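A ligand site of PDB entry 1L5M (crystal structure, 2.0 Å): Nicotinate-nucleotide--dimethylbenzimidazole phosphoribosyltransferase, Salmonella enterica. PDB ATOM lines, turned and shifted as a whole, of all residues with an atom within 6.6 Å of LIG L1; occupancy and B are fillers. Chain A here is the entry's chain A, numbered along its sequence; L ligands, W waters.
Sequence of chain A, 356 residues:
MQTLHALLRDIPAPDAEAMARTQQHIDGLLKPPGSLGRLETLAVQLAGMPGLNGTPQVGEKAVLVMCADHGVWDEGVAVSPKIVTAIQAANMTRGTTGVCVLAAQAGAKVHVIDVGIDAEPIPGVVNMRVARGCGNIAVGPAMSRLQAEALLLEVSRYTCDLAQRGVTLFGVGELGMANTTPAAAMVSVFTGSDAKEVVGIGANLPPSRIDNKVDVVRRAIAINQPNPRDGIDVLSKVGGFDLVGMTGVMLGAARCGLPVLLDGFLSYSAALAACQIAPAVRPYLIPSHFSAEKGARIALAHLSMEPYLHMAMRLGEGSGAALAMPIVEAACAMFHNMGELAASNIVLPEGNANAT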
ATOM      1  N   GLU A 174      33.647  21.629   6.239  1.00  0.00           N
ATOM      2  CA  GLU A 174      33.038  21.208   7.486  1.00  0.00           C
ATOM      3  C   GLU A 174      32.022  20.078   7.323  1.00  0.00           C
ATOM      4  O   GLU A 174      31.679  19.683   6.206  1.00  0.00           O
ATOM      5  CB  GLU A 174      32.343  22.403   8.159  1.00  0.00           C
ATOM      6  CG  GLU A 174      31.540  23.280   7.191  1.00  0.00           C
ATOM      7  CD  GLU A 174      30.482  22.485   6.436  1.00  0.00           C
ATOM      8  OE1 GLU A 174      29.597  21.902   7.105  1.00  0.00           O
ATOM      9  OE2 GLU A 174      30.540  22.427   5.193  1.00  0.00           O
ATOM     10  N   ASN A 179      24.558  22.767  11.365  1.00  0.00           N
ATOM     11  CA  ASN A 179      25.467  23.907  11.410  1.00  0.00           C
ATOM     12  C   ASN A 179      25.115  25.150  10.587  1.00  0.00           C
ATOM     13  O   ASN A 179      25.755  26.184  10.778  1.00  0.00           O
ATOM     14  CB  ASN A 179      26.950  23.494  11.205  1.00  0.00           C
ATOM     15  CG  ASN A 179      27.305  23.048   9.789  1.00  0.00           C
ATOM     16  OD1 ASN A 179      26.501  23.134   8.858  1.00  0.00           O
ATOM     17  ND2 ASN A 179      28.542  22.564   9.626  1.00  0.00           N
ATOM     18  N   THR A 180      24.105  25.091   9.711  1.00  0.00           N
ATOM     19  CA  THR A 180      23.753  26.308   8.985  1.00  0.00           C
ATOM     20  C   THR A 180      22.957  27.240   9.905  1.00  0.00           C
ATOM     21  O   THR A 180      22.745  28.403   9.582  1.00  0.00           O
ATOM     22  CB  THR A 180      22.946  26.050   7.679  1.00  0.00           C
ATOM     23  OG1 THR A 180      21.697  25.416   7.990  1.00  0.00           O
ATOM     24  CG2 THR A 180      23.751  25.172   6.722  1.00  0.00           C
ATOM     25  N   ILE A 201      17.513  27.112   3.774  1.00  0.00           N
ATOM     26  CA  ILE A 201      17.024  25.739   3.909  1.00  0.00           C
ATOM     27  C   ILE A 201      18.105  24.700   4.279  1.00  0.00           C
ATOM     28  O   ILE A 201      17.800  23.513   4.420  1.00  0.00           O
ATOM     29  CB  ILE A 201      16.310  25.319   2.614  1.00  0.00           C
ATOM     30  N   GLY A 202      19.357  25.144   4.426  1.00  0.00           N
ATOM     31  CA  GLY A 202      20.413  24.204   4.799  1.00  0.00           C
ATOM     32  C   GLY A 202      20.362  22.951   3.926  1.00  0.00           C
ATOM     33  O   GLY A 202      20.252  23.051   2.701  1.00  0.00           O
ATOM     34  N   ALA A 203      20.427  21.780   4.549  1.00  0.00           N
ATOM     35  CA  ALA A 203      20.389  20.523   3.817  1.00  0.00           C
ATOM     36  C   ALA A 203      18.940  20.075   3.639  1.00  0.00           C
ATOM     37  O   ALA A 203      18.438  19.213   4.364  1.00  0.00           O
ATOM     38  CB  ALA A 203      21.206  19.449   4.574  1.00  0.00           C
ATOM     39  N   ASN A 204      18.260  20.694   2.686  1.00  0.00           N
ATOM     40  CA  ASN A 204      16.861  20.378   2.384  1.00  0.00           C
ATOM     41  C   ASN A 204      15.850  20.488   3.529  1.00  0.00           C
ATOM     42  O   ASN A 204      15.005  19.619   3.679  1.00  0.00           O
ATOM     43  CB  ASN A 204      16.763  18.980   1.775  1.00  0.00           C
ATOM     44  CG  ASN A 204      17.455  18.883   0.434  1.00  0.00           C
ATOM     45  OD1 ASN A 204      17.661  19.902  -0.233  1.00  0.00           O
ATOM     46  ND2 ASN A 204      17.794  17.669   0.002  1.00  0.00           N
ATOM     47  N   ASP A 263      34.910  27.969   1.009  1.00  0.00           N
ATOM     48  CA  ASP A 263      33.976  27.007   0.435  1.00  0.00           C
ATOM     49  C   ASP A 263      32.643  27.690   0.257  1.00  0.00           C
ATOM     50  O   ASP A 263      32.518  28.608  -0.561  1.00  0.00           O
ATOM     51  CB  ASP A 263      33.845  25.756   1.326  1.00  0.00           C
ATOM     52  CG  ASP A 263      32.951  24.673   0.696  1.00  0.00           C
ATOM     53  OD1 ASP A 263      32.892  24.576  -0.563  1.00  0.00           O
ATOM     54  OD2 ASP A 263      32.327  23.899   1.447  1.00  0.00           O
ATOM     55  N   GLY A 264      31.646  27.252   1.021  1.00  0.00           N
ATOM     56  CA  GLY A 264      30.323  27.826   0.910  1.00  0.00           C
ATOM     57  C   GLY A 264      29.879  28.686   2.092  1.00  0.00           C
ATOM     58  O   GLY A 264      30.689  29.327   2.759  1.00  0.00           O
ATOM     59  N   PHE A 265      28.574  28.654   2.349  1.00  0.00           N
ATOM     60  CA  PHE A 265      27.962  29.452   3.415  1.00  0.00           C
ATOM     61  C   PHE A 265      28.607  29.328   4.794  1.00  0.00           C
ATOM     62  O   PHE A 265      28.861  30.327   5.460  1.00  0.00           O
ATOM     63  CB  PHE A 265      26.461  29.144   3.508  1.00  0.00           C
ATOM     64  CG  PHE A 265      25.706  30.077   4.398  1.00  0.00           C
ATOM     65  CD1 PHE A 265      25.112  29.626   5.556  1.00  0.00           C
ATOM     66  CD2 PHE A 265      25.625  31.431   4.091  1.00  0.00           C
ATOM     67  CE1 PHE A 265      24.439  30.505   6.404  1.00  0.00           C
ATOM     68  CE2 PHE A 265      24.968  32.324   4.933  1.00  0.00           C
ATOM     69  CZ  PHE A 265      24.371  31.855   6.103  1.00  0.00           C
ATOM     70  N   LEU A 266      28.865  28.098   5.230  1.00  0.00           N
ATOM     71  CA  LEU A 266      29.501  27.906   6.531  1.00  0.00           C
ATOM     72  C   LEU A 266      30.862  28.603   6.579  1.00  0.00           C
ATOM     73  O   LEU A 266      31.224  29.223   7.583  1.00  0.00           O
ATOM     74  CB  LEU A 266      29.712  26.414   6.836  1.00  0.00           C
ATOM     75  CG  LEU A 266      28.523  25.472   7.073  1.00  0.00           C
ATOM     76  CD1 LEU A 266      27.449  26.178   7.928  1.00  0.00           C
ATOM     77  CD2 LEU A 266      27.928  25.029   5.758  1.00  0.00           C
ATOM     78  N   SER A 267      31.617  28.493   5.498  1.00  0.00           N
ATOM     79  CA  SER A 267      32.944  29.088   5.438  1.00  0.00           C
ATOM     80  C   SER A 267      32.883  30.617   5.424  1.00  0.00           C
ATOM     81  O   SER A 267      33.800  31.270   5.912  1.00  0.00           O
ATOM     82  CB  SER A 267      33.707  28.576   4.197  1.00  0.00           C
ATOM     83  OG  SER A 267      33.327  29.283   3.031  1.00  0.00           O
ATOM     84  N   TYR A 268      31.808  31.176   4.858  1.00  0.00           N
ATOM     85  CA  TYR A 268      31.657  32.637   4.826  1.00  0.00           C
ATOM     86  C   TYR A 268      31.503  33.146   6.265  1.00  0.00           C
ATOM     87  O   TYR A 268      32.071  34.161   6.626  1.00  0.00           O
ATOM     88  CB  TYR A 268      30.413  33.090   4.048  1.00  0.00           C
ATOM     89  CG  TYR A 268      30.292  32.668   2.596  1.00  0.00           C
ATOM     90  CD1 TYR A 268      29.021  32.619   1.997  1.00  0.00           C
ATOM     91  CD2 TYR A 268      31.398  32.240   1.859  1.00  0.00           C
ATOM     92  CE1 TYR A 268      28.858  32.138   0.704  1.00  0.00           C
ATOM     93  CE2 TYR A 268      31.240  31.766   0.545  1.00  0.00           C
ATOM     94  CZ  TYR A 268      29.958  31.716  -0.018  1.00  0.00           C
ATOM     95  OH  TYR A 268      29.758  31.167  -1.260  1.00  0.00           O
ATOM     96  N   HIS A 289      33.148  29.309  -4.786  1.00  0.00           N
ATOM     97  CA  HIS A 289      31.833  29.360  -5.410  1.00  0.00           C
ATOM     98  C   HIS A 289      30.805  30.191  -4.657  1.00  0.00           C
ATOM     99  O   HIS A 289      31.018  30.597  -3.507  1.00  0.00           O
ATOM    100  CB  HIS A 289      31.315  27.918  -5.622  1.00  0.00           C
ATOM    101  CG  HIS A 289      30.722  27.295  -4.395  1.00  0.00           C
ATOM    102  ND1 HIS A 289      31.478  26.978  -3.287  1.00  0.00           N
ATOM    103  CD2 HIS A 289      29.456  26.899  -4.125  1.00  0.00           C
ATOM    104  CE1 HIS A 289      30.698  26.410  -2.377  1.00  0.00           C
ATOM    105  NE2 HIS A 289      29.472  26.348  -2.864  1.00  0.00           N
ATOM    106  N   SER A 291      27.490  30.021  -2.950  1.00  0.00           N
ATOM    107  CA  SER A 291      26.528  29.111  -2.339  1.00  0.00           C
ATOM    108  C   SER A 291      25.069  29.430  -2.655  1.00  0.00           C
ATOM    109  O   SER A 291      24.690  30.601  -2.753  1.00  0.00           O
ATOM    110  CB  SER A 291      26.686  29.103  -0.808  1.00  0.00           C
ATOM    111  OG  SER A 291      25.686  28.296  -0.201  1.00  0.00           O
ATOM    112  N   ALA A 292      24.264  28.382  -2.773  1.00  0.00           N
ATOM    113  CA  ALA A 292      22.828  28.538  -3.042  1.00  0.00           C
ATOM    114  C   ALA A 292      22.055  28.840  -1.742  1.00  0.00           C
ATOM    115  O   ALA A 292      20.835  28.932  -1.739  1.00  0.00           O
ATOM    116  CB  ALA A 292      22.297  27.275  -3.684  1.00  0.00           C
ATOM    117  N   GLU A 293      22.762  28.958  -0.626  1.00  0.00           N
ATOM    118  CA  GLU A 293      22.118  29.288   0.645  1.00  0.00           C
ATOM    119  C   GLU A 293      21.611  30.749   0.571  1.00  0.00           C
ATOM    120  O   GLU A 293      22.257  31.632   0.015  1.00  0.00           O
ATOM    121  CB  GLU A 293      23.153  29.106   1.774  1.00  0.00           C
ATOM    122  CG  GLU A 293      22.668  29.278   3.195  1.00  0.00           C
ATOM    123  CD  GLU A 293      21.761  28.167   3.728  1.00  0.00           C
ATOM    124  OE1 GLU A 293      21.436  28.213   4.928  1.00  0.00           O
ATOM    125  OE2 GLU A 293      21.369  27.239   2.987  1.00  0.00           O
ATOM    126  N   MET A 313      25.740  25.316  -5.849  1.00  0.00           N
ATOM    127  CA  MET A 313      26.103  24.250  -4.917  1.00  0.00           C
ATOM    128  C   MET A 313      25.776  24.581  -3.470  1.00  0.00           C
ATOM    129  O   MET A 313      25.841  25.737  -3.054  1.00  0.00           O
ATOM    130  CB  MET A 313      27.582  23.911  -5.079  1.00  0.00           C
ATOM    131  CG  MET A 313      27.854  22.954  -6.230  1.00  0.00           C
ATOM    132  SD  MET A 313      29.566  22.962  -6.755  1.00  0.00           S
ATOM    133  CE  MET A 313      30.366  22.365  -5.277  1.00  0.00           C
ATOM    134  N   ARG A 314      25.433  23.547  -2.709  1.00  0.00           N
ATOM    135  CA  ARG A 314      25.068  23.725  -1.311  1.00  0.00           C
ATOM    136  C   ARG A 314      25.307  22.449  -0.524  1.00  0.00           C
ATOM    137  O   ARG A 314      24.488  22.033   0.302  1.00  0.00           O
ATOM    138  CB  ARG A 314      23.584  24.135  -1.213  1.00  0.00           C
ATOM    139  CG  ARG A 314      22.607  23.221  -1.945  1.00  0.00           C
ATOM    140  CD  ARG A 314      21.174  23.804  -1.846  1.00  0.00           C
ATOM    141  NE  ARG A 314      20.202  23.176  -2.743  1.00  0.00           N
ATOM    142  CZ  ARG A 314      19.623  21.998  -2.530  1.00  0.00           C
ATOM    143  NH1 ARG A 314      19.899  21.314  -1.438  1.00  0.00           N
ATOM    144  NH2 ARG A 314      18.766  21.506  -3.424  1.00  0.00           N
ATOM    145  N   LEU A 315      26.442  21.810  -0.770  1.00  0.00           N
ATOM    146  CA  LEU A 315      26.768  20.574  -0.095  1.00  0.00           C
ATOM    147  C   LEU A 315      27.665  20.803   1.120  1.00  0.00           C
ATOM    148  O   LEU A 315      27.499  20.153   2.134  1.00  0.00           O
ATOM    149  CB  LEU A 315      27.446  19.604  -1.059  1.00  0.00           C
ATOM    150  CG  LEU A 315      28.089  18.343  -0.437  1.00  0.00           C
ATOM    151  CD1 LEU A 315      27.020  17.490   0.232  1.00  0.00           C
ATOM    152  CD2 LEU A 315      28.800  17.544  -1.534  1.00  0.00           C
ATOM    153  N   GLY A 316      28.621  21.718   1.000  1.00  0.00           N
ATOM    154  CA  GLY A 316      29.536  21.935   2.114  1.00  0.00           C
ATOM    155  C   GLY A 316      30.682  20.936   1.968  1.00  0.00           C
ATOM    156  O   GLY A 316      30.996  20.511   0.853  1.00  0.00           O
ATOM    157  N   GLU A 317      31.284  20.554   3.088  1.00  0.00           N
ATOM    158  CA  GLU A 317      32.407  19.609   3.118  1.00  0.00           C
ATOM    159  C   GLU A 317      33.702  20.140   2.533  1.00  0.00           C
ATOM    160  O   GLU A 317      34.746  19.473   2.613  1.00  0.00           O
ATOM    161  CB  GLU A 317      32.058  18.324   2.355  1.00  0.00           C
ATOM    162  CG  GLU A 317      30.684  17.750   2.682  1.00  0.00           C
ATOM    163  CD  GLU A 317      30.468  16.399   2.023  1.00  0.00           C
ATOM    164  OE1 GLU A 317      31.350  15.987   1.237  1.00  0.00           O
ATOM    165  OE2 GLU A 317      29.422  15.769   2.280  1.00  0.00           O
ATOM    166  N   GLY A 318      33.637  21.311   1.924  1.00  0.00           N
ATOM    167  CA  GLY A 318      34.823  21.869   1.294  1.00  0.00           C
ATOM    168  C   GLY A 318      34.803  21.433  -0.169  1.00  0.00           C
ATOM    169  O   GLY A 318      35.827  21.516  -0.861  1.00  0.00           O
ATOM    170  N   SER A 319      33.641  20.989  -0.638  1.00  0.00           N
ATOM    171  CA  SER A 319      33.491  20.531  -2.021  1.00  0.00           C
ATOM    172  C   SER A 319      33.733  21.640  -3.036  1.00  0.00           C
ATOM    173  O   SER A 319      34.297  21.401  -4.096  1.00  0.00           O
ATOM    174  CB  SER A 319      32.099  19.921  -2.231  1.00  0.00           C
ATOM    175  OG  SER A 319      31.084  20.836  -1.847  1.00  0.00           O
HETATM  176  N1  LIG L   1      25.310  22.767   3.607  1.00  0.00           N
HETATM  177  C1  LIG L   1      26.385  23.505   3.148  1.00  0.00           C
HETATM  178  C2  LIG L   1      26.103  24.677   2.423  1.00  0.00           C
HETATM  179  C3  LIG L   1      24.715  25.122   2.187  1.00  0.00           C
HETATM  180  C4  LIG L   1      23.720  24.273   2.720  1.00  0.00           C
HETATM  181  C5  LIG L   1      23.940  23.083   3.444  1.00  0.00           C
HETATM  182  C6  LIG L   1      27.273  25.525   1.900  1.00  0.00           C
HETATM  183  O1  LIG L   1      27.031  26.587   1.263  1.00  0.00           O
HETATM  184  O2  LIG L   1      28.499  25.152   2.104  1.00  0.00           O
HETATM  185  C1  LG2 L   2      26.404  16.150   4.033  1.00  0.00           C
HETATM  186  C2  LG2 L   2      25.646  17.203   4.587  1.00  0.00           C
HETATM  187  C3  LG2 L   2      24.333  16.915   5.075  1.00  0.00           C
HETATM  188  N1  LG2 L   2      23.896  15.606   4.974  1.00  0.00           N
HETATM  189  C4  LG2 L   2      24.680  14.619   4.418  1.00  0.00           C
HETATM  190  N2  LG2 L   2      25.933  14.876   3.950  1.00  0.00           N
HETATM  191  N3  LG2 L   2      27.567  16.684   3.651  1.00  0.00           N
HETATM  192  C5  LG2 L   2      27.530  17.981   3.927  1.00  0.00           C
HETATM  193  N4  LG2 L   2      26.375  18.367   4.519  1.00  0.00           N
HETATM  194  N5  LG2 L   2      24.191  13.312   4.339  1.00  0.00           N
HETATM  195  P1  LG2 L   2      21.791  21.681   8.024  1.00  0.00           P
HETATM  196  O1  LG2 L   2      22.039  22.902   8.868  1.00  0.00           O
HETATM  197  O2  LG2 L   2      20.458  21.702   7.391  1.00  0.00           O
HETATM  198  O3  LG2 L   2      21.905  20.472   8.877  1.00  0.00           O
HETATM  199  O4  LG2 L   2      22.905  21.670   6.858  1.00  0.00           O
HETATM  200  C6  LG2 L   2      24.321  21.697   7.174  1.00  0.00           C
HETATM  201  C7  LG2 L   2      24.891  20.311   6.997  1.00  0.00           C
HETATM  202  O5  LG2 L   2      24.755  19.797   5.621  1.00  0.00           O
HETATM  203  C8  LG2 L   2      26.380  20.148   7.285  1.00  0.00           C
HETATM  204  O6  LG2 L   2      26.728  18.813   7.701  1.00  0.00           O
HETATM  205  C9  LG2 L   2      26.949  20.474   5.931  1.00  0.00           C
HETATM  206  O7  LG2 L   2      28.313  20.050   5.806  1.00  0.00           O
HETATM  207  C10 LG2 L   2      25.989  19.798   4.958  1.00  0.00           C
HETATM  208  O   HOH W   1      20.900  25.352   1.132  1.00  0.00           O
HETATM  209  O   HOH W   2      30.017  24.576  -0.136  1.00  0.00           O
HETATM  210  O   HOH W   3      30.593  26.182   3.509  1.00  0.00           O
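The backbone carbonyl oxygen of Arg 314 lies close to a nitrogen (N1) of LIG L1, 3.5 Å away. Residues that only touch LIG L1: Thr 180 (3.9 Å), Gly 202 (3.6 Å), Ala 203 (3.9 Å), Gly 264 (3.5 Å), Leu 266 (3.4 Å), Glu 293 (3.8 Å), Leu 315 (3.6 Å) and Gly 316 (3.4 Å). Within 4 Å of LIG L1: Thr 180, Gly 202, Ala 203, Gly 264, Phe 265, Leu 266, Ser 291, Glu 293, Arg 314, Leu 315 and Gly 316. The nearest printed residue that does not touch LIG L1 is Asp 263 (4.1 Å).
O1 of LIG L1 sits at hydrogen-bond distance from OG of Ser 291 (2.6 Å). N of Phe 265 sits at hydrogen-bond distance from O1 of LIG L1 (2.8 Å). N of Thr 180 lies within hydrogen-bond range of O1 of LG2 L2. An oxygen (O1) of LG2 L2 sits at hydrogen-bond distance from the side-chain hydroxyl (OG1) of Thr 180 (2.7 Å). The backbone NH (N) of Ala 203 lies within hydrogen-bond range of an oxygen (O2) of LG2 L2. O of Glu 174 sits close to O7 of LG2 L2, at 3.4 Å. O7 of LG2 L2 is in hydrogen-bond range of OE1 of Glu 174, 2.6 Å away. The side-chain carboxylate (OE2) of Glu 317 is in hydrogen-bond range of a nitrogen (N3) of LG2 L2.
Water W2 lies within hydrogen-bond range of an oxygen (O2) of LIG L1, the side-chain carboxylate of Asp 263, a ring nitrogen (NE2) of His 289, the backbone NH of Gly 264 and the backbone NH of Gly 316. Water W1 bridges the side-chain carboxylate of Glu 293 (2.7 Å) and the backbone carbonyl oxygen of Gly 202 (2.9 Å).
The side-chain hydroxyl of Ser 291 is in hydrogen-bond range of the backbone NH of Glu 293. N of Ser 291 sits at hydrogen-bond distance from OH of Tyr 268, at 3.1 Å. The guanidinium group (NH1) of Arg 314 is in hydrogen-bond range of the side-chain amide oxygen (OD1) of Asn 204, 2.9 Å away. O of Gly 316 lies within hydrogen-bond range of OG of Ser 319, 2.7 Å away. The backbone carbonyl oxygen of Gly 264 sits at hydrogen-bond distance from the side-chain hydroxyl of Ser 267 (2.7 Å). N of Gly 202 is in hydrogen-bond range of OE2 of Glu 293, 3.2 Å away.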
